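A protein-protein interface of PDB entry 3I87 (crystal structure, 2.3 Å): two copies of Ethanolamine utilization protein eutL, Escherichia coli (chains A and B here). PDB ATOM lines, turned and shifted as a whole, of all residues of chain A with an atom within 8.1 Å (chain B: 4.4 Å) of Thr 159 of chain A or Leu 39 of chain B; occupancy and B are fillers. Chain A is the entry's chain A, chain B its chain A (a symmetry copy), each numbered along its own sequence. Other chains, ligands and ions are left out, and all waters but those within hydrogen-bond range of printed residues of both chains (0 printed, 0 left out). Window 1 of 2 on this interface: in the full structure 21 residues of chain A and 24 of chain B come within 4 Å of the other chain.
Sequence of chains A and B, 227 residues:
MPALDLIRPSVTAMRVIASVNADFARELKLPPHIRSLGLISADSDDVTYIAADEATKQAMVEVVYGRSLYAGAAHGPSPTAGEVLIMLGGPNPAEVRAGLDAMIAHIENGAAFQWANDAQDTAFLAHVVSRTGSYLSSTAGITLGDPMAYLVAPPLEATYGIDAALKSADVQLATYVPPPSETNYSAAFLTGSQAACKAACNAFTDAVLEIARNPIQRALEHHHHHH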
ATOM      1  N   ALA A 153     -22.301   6.839 -20.922  1.00  0.00           N
ATOM      2  CA  ALA A 153     -21.405   7.223 -19.830  1.00  0.00           C
ATOM      3  C   ALA A 153     -20.801   8.592 -20.118  1.00  0.00           C
ATOM      4  O   ALA A 153     -20.971   9.116 -21.215  1.00  0.00           O
ATOM      5  CB  ALA A 153     -20.303   6.188 -19.667  1.00  0.00           C
ATOM      6  N   PRO A 154     -20.092   9.178 -19.136  1.00  0.00           N
ATOM      7  CA  PRO A 154     -19.296  10.366 -19.447  1.00  0.00           C
ATOM      8  C   PRO A 154     -18.201  10.057 -20.477  1.00  0.00           C
ATOM      9  O   PRO A 154     -17.641   8.964 -20.455  1.00  0.00           O
ATOM     10  CB  PRO A 154     -18.698  10.757 -18.093  1.00  0.00           C
ATOM     11  CG  PRO A 154     -19.647  10.200 -17.093  1.00  0.00           C
ATOM     12  CD  PRO A 154     -20.126   8.909 -17.688  1.00  0.00           C
ATOM     13  N   PRO A 155     -17.898  11.023 -21.365  1.00  0.00           N
ATOM     14  CA  PRO A 155     -17.153  10.813 -22.616  1.00  0.00           C
ATOM     15  C   PRO A 155     -15.843  10.025 -22.518  1.00  0.00           C
ATOM     16  O   PRO A 155     -15.558   9.228 -23.417  1.00  0.00           O
ATOM     17  CB  PRO A 155     -16.891  12.243 -23.130  1.00  0.00           C
ATOM     18  CG  PRO A 155     -17.235  13.153 -22.009  1.00  0.00           C
ATOM     19  CD  PRO A 155     -18.244  12.442 -21.174  1.00  0.00           C
ATOM     20  N   LEU A 156     -15.053  10.234 -21.466  1.00  0.00           N
ATOM     21  CA  LEU A 156     -13.810   9.468 -21.304  1.00  0.00           C
ATOM     22  C   LEU A 156     -14.132   8.018 -20.968  1.00  0.00           C
ATOM     23  O   LEU A 156     -13.595   7.102 -21.595  1.00  0.00           O
ATOM     24  CB  LEU A 156     -12.890  10.073 -20.238  1.00  0.00           C
ATOM     25  CG  LEU A 156     -11.479   9.461 -20.192  1.00  0.00           C
ATOM     26  CD1 LEU A 156     -10.417  10.479 -19.756  1.00  0.00           C
ATOM     27  CD2 LEU A 156     -11.437   8.233 -19.298  1.00  0.00           C
ATOM     28  N   GLU A 157     -15.010   7.823 -19.982  1.00  0.00           N
ATOM     29  CA  GLU A 157     -15.473   6.487 -19.598  1.00  0.00           C
ATOM     30  C   GLU A 157     -16.168   5.763 -20.750  1.00  0.00           C
ATOM     31  O   GLU A 157     -15.981   4.559 -20.926  1.00  0.00           O
ATOM     32  CB  GLU A 157     -16.430   6.554 -18.398  1.00  0.00           C
ATOM     33  CG  GLU A 157     -15.752   6.774 -17.050  1.00  0.00           C
ATOM     34  CD  GLU A 157     -15.743   8.226 -16.596  1.00  0.00           C
ATOM     35  OE1 GLU A 157     -15.578   9.141 -17.444  1.00  0.00           O
ATOM     36  OE2 GLU A 157     -15.891   8.447 -15.372  1.00  0.00           O
ATOM     37  N   ALA A 158     -16.971   6.492 -21.523  1.00  0.00           N
ATOM     38  CA  ALA A 158     -17.657   5.914 -22.676  1.00  0.00           C
ATOM     39  C   ALA A 158     -16.655   5.381 -23.700  1.00  0.00           C
ATOM     40  O   ALA A 158     -16.762   4.237 -24.134  1.00  0.00           O
ATOM     41  CB  ALA A 158     -18.589   6.935 -23.323  1.00  0.00           C
ATOM     42  N   THR A 159     -15.673   6.205 -24.060  1.00  0.00           N
ATOM     43  CA  THR A 159     -14.658   5.839 -25.058  1.00  0.00           C
ATOM     44  C   THR A 159     -13.895   4.585 -24.655  1.00  0.00           C
ATOM     45  O   THR A 159     -13.756   3.649 -25.444  1.00  0.00           O
ATOM     46  CB  THR A 159     -13.639   6.981 -25.269  1.00  0.00           C
ATOM     47  OG1 THR A 159     -14.320   8.151 -25.736  1.00  0.00           O
ATOM     48  CG2 THR A 159     -12.574   6.584 -26.281  1.00  0.00           C
ATOM     49  N   TYR A 160     -13.406   4.581 -23.420  1.00  0.00           N
ATOM     50  CA  TYR A 160     -12.645   3.457 -22.886  1.00  0.00           C
ATOM     51  C   TYR A 160     -13.516   2.203 -22.797  1.00  0.00           C
ATOM     52  O   TYR A 160     -13.081   1.111 -23.168  1.00  0.00           O
ATOM     53  CB  TYR A 160     -12.088   3.817 -21.504  1.00  0.00           C
ATOM     54  CG  TYR A 160     -10.947   2.943 -21.030  1.00  0.00           C
ATOM     55  CD1 TYR A 160      -9.663   3.101 -21.545  1.00  0.00           C
ATOM     56  CD2 TYR A 160     -11.143   1.977 -20.045  1.00  0.00           C
ATOM     57  CE1 TYR A 160      -8.602   2.312 -21.102  1.00  0.00           C
ATOM     58  CE2 TYR A 160     -10.091   1.182 -19.597  1.00  0.00           C
ATOM     59  CZ  TYR A 160      -8.826   1.354 -20.129  1.00  0.00           C
ATOM     60  OH  TYR A 160      -7.785   0.570 -19.691  1.00  0.00           O
ATOM     61  N   GLY A 161     -14.742   2.373 -22.309  1.00  0.00           N
ATOM     62  CA  GLY A 161     -15.703   1.275 -22.202  1.00  0.00           C
ATOM     63  C   GLY A 161     -16.114   0.650 -23.528  1.00  0.00           C
ATOM     64  O   GLY A 161     -16.260  -0.569 -23.616  1.00  0.00           O
ATOM     65  N   ILE A 162     -16.314   1.482 -24.553  1.00  0.00           N
ATOM     66  CA  ILE A 162     -16.667   1.007 -25.900  1.00  0.00           C
ATOM     67  C   ILE A 162     -15.561   0.125 -26.482  1.00  0.00           C
ATOM     68  O   ILE A 162     -15.835  -0.937 -27.038  1.00  0.00           O
ATOM     69  CB  ILE A 162     -16.934   2.190 -26.869  1.00  0.00           C
ATOM     70  CG1 ILE A 162     -18.258   2.881 -26.534  1.00  0.00           C
ATOM     71  CG2 ILE A 162     -16.983   1.716 -28.308  1.00  0.00           C
ATOM     72  CD1 ILE A 162     -18.385   4.271 -27.157  1.00  0.00           C
ATOM     73  N   ASP A 163     -14.315   0.575 -26.347  1.00  0.00           N
ATOM     74  CA  ASP A 163     -13.147  -0.199 -26.775  1.00  0.00           C
ATOM     75  C   ASP A 163     -13.078  -1.540 -26.035  1.00  0.00           C
ATOM     76  O   ASP A 163     -12.779  -2.573 -26.637  1.00  0.00           O
ATOM     77  CB  ASP A 163     -11.863   0.609 -26.534  1.00  0.00           C
ATOM     78  CG  ASP A 163     -10.604  -0.152 -26.918  1.00  0.00           C
ATOM     79  OD1 ASP A 163     -10.327  -0.285 -28.132  1.00  0.00           O
ATOM     80  OD2 ASP A 163      -9.883  -0.607 -26.002  1.00  0.00           O
ATOM     81  N   ALA A 164     -13.364  -1.512 -24.735  1.00  0.00           N
ATOM     82  CA  ALA A 164     -13.355  -2.716 -23.904  1.00  0.00           C
ATOM     83  C   ALA A 164     -14.478  -3.683 -24.285  1.00  0.00           C
ATOM     84  O   ALA A 164     -14.268  -4.898 -24.326  1.00  0.00           O
ATOM     85  CB  ALA A 164     -13.453  -2.340 -22.431  1.00  0.00           C
ATOM     86  N   ALA A 165     -15.665  -3.136 -24.560  1.00  0.00           N
ATOM     87  CA  ALA A 165     -16.823  -3.929 -24.978  1.00  0.00           C
ATOM     88  C   ALA A 165     -16.569  -4.656 -26.299  1.00  0.00           C
ATOM     89  O   ALA A 165     -16.856  -5.849 -26.421  1.00  0.00           O
ATOM     90  CB  ALA A 165     -18.058  -3.037 -25.104  1.00  0.00           C
ATOM     91  N   LEU A 166     -16.030  -3.935 -27.280  1.00  0.00           N
ATOM     92  CA  LEU A 166     -15.725  -4.516 -28.589  1.00  0.00           C
ATOM     93  C   LEU A 166     -14.685  -5.635 -28.486  1.00  0.00           C
ATOM     94  O   LEU A 166     -14.734  -6.595 -29.249  1.00  0.00           O
ATOM     95  CB  LEU A 166     -15.251  -3.434 -29.571  1.00  0.00           C
ATOM     96  CG  LEU A 166     -16.323  -2.456 -30.077  1.00  0.00           C
ATOM     97  CD1 LEU A 166     -15.697  -1.190 -30.664  1.00  0.00           C
ATOM     98  CD2 LEU A 166     -17.233  -3.127 -31.107  1.00  0.00           C
ATOM     99  N   TYR A 176     -21.044   5.437 -35.021  1.00  0.00           N
ATOM    100  CA  TYR A 176     -20.315   6.224 -34.026  1.00  0.00           C
ATOM    101  C   TYR A 176     -20.153   7.688 -34.429  1.00  0.00           C
ATOM    102  O   TYR A 176     -19.625   7.996 -35.501  1.00  0.00           O
ATOM    103  CB  TYR A 176     -18.935   5.614 -33.768  1.00  0.00           C
ATOM    104  CG  TYR A 176     -18.169   6.309 -32.660  1.00  0.00           C
ATOM    105  CD1 TYR A 176     -17.110   7.167 -32.951  1.00  0.00           C
ATOM    106  CD2 TYR A 176     -18.516   6.124 -31.324  1.00  0.00           C
ATOM    107  CE1 TYR A 176     -16.408   7.812 -31.938  1.00  0.00           C
ATOM    108  CE2 TYR A 176     -17.822   6.766 -30.303  1.00  0.00           C
ATOM    109  CZ  TYR A 176     -16.769   7.607 -30.617  1.00  0.00           C
ATOM    110  OH  TYR A 176     -16.075   8.246 -29.615  1.00  0.00           O
ATOM    111  N   PRO A 178     -18.340  10.950 -32.511  1.00  0.00           N
ATOM    112  CA  PRO A 178     -17.548  11.269 -31.312  1.00  0.00           C
ATOM    113  C   PRO A 178     -18.185  12.349 -30.425  1.00  0.00           C
ATOM    114  O   PRO A 178     -19.062  13.080 -30.892  1.00  0.00           O
ATOM    115  CB  PRO A 178     -16.212  11.768 -31.883  1.00  0.00           C
ATOM    116  CG  PRO A 178     -16.181  11.311 -33.298  1.00  0.00           C
ATOM    117  CD  PRO A 178     -17.602  11.262 -33.749  1.00  0.00           C
ATOM    118  N   PRO A 179     -17.752  12.444 -29.151  1.00  0.00           N
ATOM    119  CA  PRO A 179     -18.239  13.488 -28.241  1.00  0.00           C
ATOM    120  C   PRO A 179     -18.029  14.913 -28.784  1.00  0.00           C
ATOM    121  O   PRO A 179     -16.990  15.183 -29.392  1.00  0.00           O
ATOM    122  CB  PRO A 179     -17.398  13.273 -26.979  1.00  0.00           C
ATOM    123  CG  PRO A 179     -17.034  11.842 -27.010  1.00  0.00           C
ATOM    124  CD  PRO A 179     -16.866  11.490 -28.457  1.00  0.00           C
ATOM    125  N   SER A 186     -22.024  10.783 -23.330  1.00  0.00           N
ATOM    126  CA  SER A 186     -22.075  10.321 -24.720  1.00  0.00           C
ATOM    127  C   SER A 186     -22.583   8.878 -24.782  1.00  0.00           C
ATOM    128  O   SER A 186     -22.422   8.111 -23.830  1.00  0.00           O
ATOM    129  CB  SER A 186     -20.702  10.442 -25.385  1.00  0.00           C
ATOM    130  OG  SER A 186     -19.796   9.483 -24.882  1.00  0.00           O
ATOM    131  N   ALA A 187     -23.200   8.523 -25.908  1.00  0.00           N
ATOM    132  CA  ALA A 187     -23.839   7.219 -26.076  1.00  0.00           C
ATOM    133  C   ALA A 187     -23.207   6.419 -27.214  1.00  0.00           C
ATOM    134  O   ALA A 187     -22.569   6.983 -28.100  1.00  0.00           O
ATOM    135  CB  ALA A 187     -25.331   7.397 -26.329  1.00  0.00           C
ATOM    136  N   ALA A 188     -23.397   5.103 -27.173  1.00  0.00           N
ATOM    137  CA  ALA A 188     -22.946   4.207 -28.234  1.00  0.00           C
ATOM    138  C   ALA A 188     -23.921   3.045 -28.372  1.00  0.00           C
ATOM    139  O   ALA A 188     -24.460   2.573 -27.373  1.00  0.00           O
ATOM    140  CB  ALA A 188     -21.550   3.689 -27.933  1.00  0.00           C
ATOM    141  N   PHE A 204     -18.456  -3.215 -20.553  1.00  0.00           N
ATOM    142  CA  PHE A 204     -18.610  -1.758 -20.502  1.00  0.00           C
ATOM    143  C   PHE A 204     -18.736  -1.287 -19.049  1.00  0.00           C
ATOM    144  O   PHE A 204     -18.084  -0.329 -18.647  1.00  0.00           O
ATOM    145  CB  PHE A 204     -19.839  -1.334 -21.318  1.00  0.00           C
ATOM    146  CG  PHE A 204     -20.046   0.158 -21.398  1.00  0.00           C
ATOM    147  CD1 PHE A 204     -19.322   0.923 -22.298  1.00  0.00           C
ATOM    148  CD2 PHE A 204     -20.980   0.790 -20.588  1.00  0.00           C
ATOM    149  CE1 PHE A 204     -19.512   2.293 -22.382  1.00  0.00           C
ATOM    150  CE2 PHE A 204     -21.182   2.159 -20.669  1.00  0.00           C
ATOM    151  CZ  PHE A 204     -20.445   2.912 -21.568  1.00  0.00           C
ATOM    152  N   ALA A 207     -15.343  -1.468 -17.040  1.00  0.00           N
ATOM    153  CA  ALA A 207     -14.457  -0.356 -17.399  1.00  0.00           C
ATOM    154  C   ALA A 207     -14.885   0.968 -16.748  1.00  0.00           C
ATOM    155  O   ALA A 207     -14.040   1.743 -16.293  1.00  0.00           O
ATOM    156  CB  ALA A 207     -14.388  -0.201 -18.919  1.00  0.00           C
ATOM    157  N   VAL A 208     -16.191   1.221 -16.699  1.00  0.00           N
ATOM    158  CA  VAL A 208     -16.709   2.452 -16.098  1.00  0.00           C
ATOM    159  C   VAL A 208     -16.475   2.464 -14.585  1.00  0.00           C
ATOM    160  O   VAL A 208     -16.042   3.473 -14.025  1.00  0.00           O
ATOM    161  CB  VAL A 208     -18.214   2.639 -16.401  1.00  0.00           C
ATOM    162  CG1 VAL A 208     -18.774   3.847 -15.654  1.00  0.00           C
ATOM    163  CG2 VAL A 208     -18.440   2.787 -17.897  1.00  0.00           C
ATOM    164  N   ILE A 211     -12.698   3.131 -13.803  1.00  0.00           N
ATOM    165  CA  ILE A 211     -12.317   4.538 -13.937  1.00  0.00           C
ATOM    166  C   ILE A 211     -12.952   5.380 -12.826  1.00  0.00           C
ATOM    167  O   ILE A 211     -12.307   6.277 -12.281  1.00  0.00           O
ATOM    168  CB  ILE A 211     -12.692   5.108 -15.325  1.00  0.00           C
ATOM    169  CG1 ILE A 211     -11.891   4.402 -16.420  1.00  0.00           C
ATOM    170  CG2 ILE A 211     -12.424   6.608 -15.384  1.00  0.00           C
ATOM    171  CD1 ILE A 211     -12.342   4.739 -17.821  1.00  0.00           C
ATOM    172  N   PRO A 215      -9.720   7.283 -11.232  1.00  0.00           N
ATOM    173  CA  PRO A 215      -9.711   8.033 -12.490  1.00  0.00           C
ATOM    174  C   PRO A 215      -8.314   8.453 -12.956  1.00  0.00           C
ATOM    175  O   PRO A 215      -8.084   8.558 -14.160  1.00  0.00           O
ATOM    176  CB  PRO A 215     -10.575   9.259 -12.177  1.00  0.00           C
ATOM    177  CG  PRO A 215     -10.475   9.434 -10.719  1.00  0.00           C
ATOM    178  CD  PRO A 215     -10.336   8.056 -10.139  1.00  0.00           C
ATOM    179  N   ALA B  13      -9.715  12.921 -15.151  1.00  0.00           N
ATOM    180  CA  ALA B  13      -9.485  11.497 -15.430  1.00  0.00           C
ATOM    181  C   ALA B  13      -8.503  11.276 -16.583  1.00  0.00           C
ATOM    182  O   ALA B  13      -8.356  12.130 -17.460  1.00  0.00           O
ATOM    183  CB  ALA B  13     -10.802  10.797 -15.725  1.00  0.00           C
ATOM    184  N   MET B  14      -7.849  10.115 -16.580  1.00  0.00           N
ATOM    185  CA  MET B  14      -6.844   9.784 -17.596  1.00  0.00           C
ATOM    186  C   MET B  14      -6.685   8.271 -17.785  1.00  0.00           C
ATOM    187  O   MET B  14      -6.618   7.521 -16.811  1.00  0.00           O
ATOM    188  CB  MET B  14      -5.493  10.396 -17.211  1.00  0.00           C
ATOM    189  CG  MET B  14      -4.466  10.423 -18.332  1.00  0.00           C
ATOM    190  SD  MET B  14      -2.924  11.229 -17.827  1.00  0.00           S
ATOM    191  CE  MET B  14      -2.085   9.874 -16.995  1.00  0.00           C
ATOM    192  N   ARG B  15      -6.620   7.844 -19.045  1.00  0.00           N
ATOM    193  CA  ARG B  15      -6.378   6.441 -19.394  1.00  0.00           C
ATOM    194  C   ARG B  15      -5.632   6.335 -20.716  1.00  0.00           C
ATOM    195  O   ARG B  15      -5.713   7.230 -21.558  1.00  0.00           O
ATOM    196  CB  ARG B  15      -7.702   5.662 -19.507  1.00  0.00           C
ATOM    197  CG  ARG B  15      -8.328   5.238 -18.187  1.00  0.00           C
ATOM    198  CD  ARG B  15      -7.402   4.319 -17.402  1.00  0.00           C
ATOM    199  NE  ARG B  15      -8.054   3.696 -16.251  1.00  0.00           N
ATOM    200  CZ  ARG B  15      -8.328   4.303 -15.097  1.00  0.00           C
ATOM    201  NH1 ARG B  15      -8.039   5.585 -14.910  1.00  0.00           N
ATOM    202  NH2 ARG B  15      -8.911   3.621 -14.118  1.00  0.00           N
ATOM    203  N   ILE B  17      -5.054   3.609 -23.997  1.00  0.00           N
ATOM    204  CA  ILE B  17      -5.398   2.405 -24.737  1.00  0.00           C
ATOM    205  C   ILE B  17      -4.175   2.014 -25.552  1.00  0.00           C
ATOM    206  O   ILE B  17      -3.846   2.672 -26.535  1.00  0.00           O
ATOM    207  CB  ILE B  17      -6.603   2.650 -25.673  1.00  0.00           C
ATOM    208  CG1 ILE B  17      -7.838   3.025 -24.841  1.00  0.00           C
ATOM    209  CG2 ILE B  17      -6.873   1.414 -26.535  1.00  0.00           C
ATOM    210  CD1 ILE B  17      -9.104   3.224 -25.655  1.00  0.00           C
ATOM    211  N   PHE B  24     -13.294  -0.128 -33.743  1.00  0.00           N
ATOM    212  CA  PHE B  24     -13.310   1.206 -33.144  1.00  0.00           C
ATOM    213  C   PHE B  24     -12.369   2.149 -33.908  1.00  0.00           C
ATOM    214  O   PHE B  24     -12.700   3.315 -34.134  1.00  0.00           O
ATOM    215  CB  PHE B  24     -12.923   1.122 -31.657  1.00  0.00           C
ATOM    216  CG  PHE B  24     -13.363   2.305 -30.819  1.00  0.00           C
ATOM    217  CD1 PHE B  24     -14.436   3.121 -31.194  1.00  0.00           C
ATOM    218  CD2 PHE B  24     -12.722   2.570 -29.619  1.00  0.00           C
ATOM    219  CE1 PHE B  24     -14.829   4.193 -30.398  1.00  0.00           C
ATOM    220  CE2 PHE B  24     -13.113   3.638 -28.819  1.00  0.00           C
ATOM    221  CZ  PHE B  24     -14.170   4.449 -29.207  1.00  0.00           C
ATOM    222  N   LEU B  37      -3.860   5.251 -28.144  1.00  0.00           N
ATOM    223  CA  LEU B  37      -4.778   6.345 -27.869  1.00  0.00           C
ATOM    224  C   LEU B  37      -4.661   6.774 -26.404  1.00  0.00           C
ATOM    225  O   LEU B  37      -4.763   5.948 -25.494  1.00  0.00           O
ATOM    226  CB  LEU B  37      -6.200   5.882 -28.185  1.00  0.00           C
ATOM    227  CG  LEU B  37      -7.228   6.881 -28.713  1.00  0.00           C
ATOM    228  CD1 LEU B  37      -6.781   7.492 -30.034  1.00  0.00           C
ATOM    229  CD2 LEU B  37      -8.576   6.172 -28.872  1.00  0.00           C
ATOM    230  N   GLY B  38      -4.417   8.065 -26.190  1.00  0.00           N
ATOM    231  CA  GLY B  38      -4.391   8.646 -24.848  1.00  0.00           C
ATOM    232  C   GLY B  38      -5.665   9.433 -24.606  1.00  0.00           C
ATOM    233  O   GLY B  38      -6.061  10.250 -25.437  1.00  0.00           O
ATOM    234  N   LEU B  39      -6.313   9.178 -23.473  1.00  0.00           N
ATOM    235  CA  LEU B  39      -7.557   9.853 -23.115  1.00  0.00           C
ATOM    236  C   LEU B  39      -7.329  10.687 -21.866  1.00  0.00           C
ATOM    237  O   LEU B  39      -6.850  10.174 -20.856  1.00  0.00           O
ATOM    238  CB  LEU B  39      -8.666   8.833 -22.851  1.00  0.00           C
ATOM    239  CG  LEU B  39      -8.909   7.771 -23.926  1.00  0.00           C
ATOM    240  CD1 LEU B  39     -10.053   6.846 -23.504  1.00  0.00           C
ATOM    241  CD2 LEU B  39      -9.205   8.424 -25.267  1.00  0.00           C
ATOM    242  N   ILE B  40      -7.664  11.971 -21.938  1.00  0.00           N
ATOM    243  CA  ILE B  40      -7.564  12.851 -20.777  1.00  0.00           C
ATOM    244  C   ILE B  40      -8.770  13.786 -20.726  1.00  0.00           C
ATOM    245  O   ILE B  40      -9.192  14.317 -21.749  1.00  0.00           O
ATOM    246  CB  ILE B  40      -6.235  13.652 -20.776  1.00  0.00           C
ATOM    247  CG1 ILE B  40      -6.097  14.467 -19.484  1.00  0.00           C
ATOM    248  CG2 ILE B  40      -6.132  14.547 -22.016  1.00  0.00           C
ATOM    249  CD1 ILE B  40      -4.683  14.976 -19.226  1.00  0.00           C
ATOM    250  N   LEU B  85     -12.972  16.343 -23.028  1.00  0.00           N
ATOM    251  CA  LEU B  85     -12.127  15.211 -23.419  1.00  0.00           C
ATOM    252  C   LEU B  85     -11.218  15.564 -24.601  1.00  0.00           C
ATOM    253  O   LEU B  85     -11.657  16.181 -25.574  1.00  0.00           O
ATOM    254  CB  LEU B  85     -12.995  13.996 -23.778  1.00  0.00           C
ATOM    255  CG  LEU B  85     -12.265  12.708 -24.184  1.00  0.00           C
ATOM    256  CD1 LEU B  85     -11.396  12.185 -23.049  1.00  0.00           C
ATOM    257  CD2 LEU B  85     -13.253  11.643 -24.630  1.00  0.00           C
ATOM    258  N   ILE B  86      -9.948  15.177 -24.494  1.00  0.00           N
ATOM    259  CA  ILE B  86      -9.037  15.166 -25.633  1.00  0.00           C
ATOM    260  C   ILE B  86      -8.538  13.734 -25.835  1.00  0.00           C
ATOM    261  O   ILE B  86      -8.201  13.041 -24.867  1.00  0.00           O
ATOM    262  CB  ILE B  86      -7.830  16.114 -25.425  1.00  0.00           C
ATOM    263  CG1 ILE B  86      -8.285  17.576 -25.449  1.00  0.00           C
ATOM    264  CG2 ILE B  86      -6.759  15.878 -26.493  1.00  0.00           C
ATOM    265  CD1 ILE B  86      -8.915  18.012 -26.762  1.00  0.00           C
ATOM    266  N   MET B  87      -8.530  13.295 -27.096  1.00  0.00           N
ATOM    267  CA  MET B  87      -7.959  12.007 -27.485  1.00  0.00           C
ATOM    268  C   MET B  87      -6.665  12.248 -28.261  1.00  0.00           C
ATOM    269  O   MET B  87      -6.692  12.826 -29.354  1.00  0.00           O
ATOM    270  CB  MET B  87      -8.931  11.211 -28.362  1.00  0.00           C
ATOM    271  CG  MET B  87     -10.329  11.044 -27.793  1.00  0.00           C
ATOM    272  SD  MET B  87     -11.287   9.802 -28.698  1.00  0.00           S
ATOM    273  CE  MET B  87     -12.922  10.529 -28.656  1.00  0.00           C
ATOM    274  N   LEU B 100       0.539  12.924 -22.990  1.00  0.00           N
ATOM    275  CA  LEU B 100      -0.281  13.155 -21.788  1.00  0.00           C
ATOM    276  C   LEU B 100       0.495  13.867 -20.674  1.00  0.00           C
ATOM    277  O   LEU B 100      -0.055  14.733 -19.999  1.00  0.00           O
ATOM    278  CB  LEU B 100      -0.855  11.837 -21.254  1.00  0.00           C
ATOM    279  CG  LEU B 100      -1.879  11.121 -22.142  1.00  0.00           C
ATOM    280  CD1 LEU B 100      -2.176   9.729 -21.589  1.00  0.00           C
ATOM    281  CD2 LEU B 100      -3.165  11.932 -22.285  1.00  0.00           C
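Of the 25 printed residues of chain A, 10 touch a printed residue of chain B.
Hydrophobic or aromatic side chains of chain B within 4 Å of the printed part of chain A: Ala 13, Ile 17, Phe 24, Leu 39 and Leu 85.
Along chain B the printed residues that touch a printed residue of chain A span positions 13 to 85.
Among the printed residues, no Asp or Glu carboxylate lies within 4 Å of a Lys or Arg side-chain nitrogen of the other chain.
Of the printed residues of chain B, Thr 159 of chain A touches Phe 24 (3.4 Å), Leu 39 (3.8 Å) and Leu 85 (3.8 Å).
Leu 39 of chain B touches just these residues of chain A: Leu 156 and Thr 159.
No residue of chain A comes within 4 Å of Gly 38 of chain B.
Of the printed residues of chain B, Tyr 160 of chain A touches Arg 15 (3.8 Å) and Ile 17 (3.8 Å).
Of the printed residues of chain B, Asp 163 of chain A touches Ile 17 (3.7 Å) and Phe 24 (3.8 Å).
Of the printed residues of chain A, Phe 24 of chain B touches Thr 159, Ile 162, Asp 163, Leu 166 and Tyr 176.
The nearest residue of chain A that does not touch Leu 39 of chain B is Tyr 160 of chain A (4.05 Å).
No position is printed for both chains.
Of the 19 pairs that touch across the chains among the printed residues, none has its exchanged pair printed and touching as well.
The backbone carbonyl oxygen of Pro 215 of chain A is in hydrogen-bond range of the guanidinium group of Arg 15 of chain B.
N of Met 14 of chain B lies within hydrogen-bond range of O of Pro 215 of chain A (2.9 Å).
N of Ile 17 of chain B lies within hydrogen-bond range of O of Leu 37 of chain B (2.8 Å).
O of Ile 40 of chain B is in hydrogen-bond range of N of Ile 86 of chain B.
The backbone carbonyl oxygen (O) of Arg 15 of chain B sits at hydrogen-bond distance from the backbone NH (N) of Leu 39 of chain B (2.8 Å).
The side-chain hydroxyl of Thr 159 of chain A is in hydrogen-bond range of the backbone carbonyl oxygen of Pro 155 of chain A (2.8 Å).
CD1 of Leu 156 of chain A touches N of Ile 40 of chain B, at 3.8 Å.
Leu 156 of chain A touches Leu 85 of chain B.
CE2 of Phe 24 of chain B touches O of Thr 159 of chain A, 3.4 Å away.
Thr 159 of chain A touches Leu 85 of chain B (OG1 to CD2, 3.8 Å).
CD1 of Tyr 160 of chain A touches CB of Arg 15 of chain B, at 3.8 Å.
Asp 163 of chain A touches Phe 24 of chain B (CB to CD2, 3.8 Å).
Phe 24 of chain B touches Leu 166 of chain A (CB to CD1, 3.7 Å).
Tyr 176 of chain A touches Phe 24 of chain B (CZ to CE1, 3.9 Å).
Ile 211 of chain A touches Arg 15 of chain B (CA to NH2, 3.5 Å).
Pro 215 of chain A touches Ala 13 of chain B.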
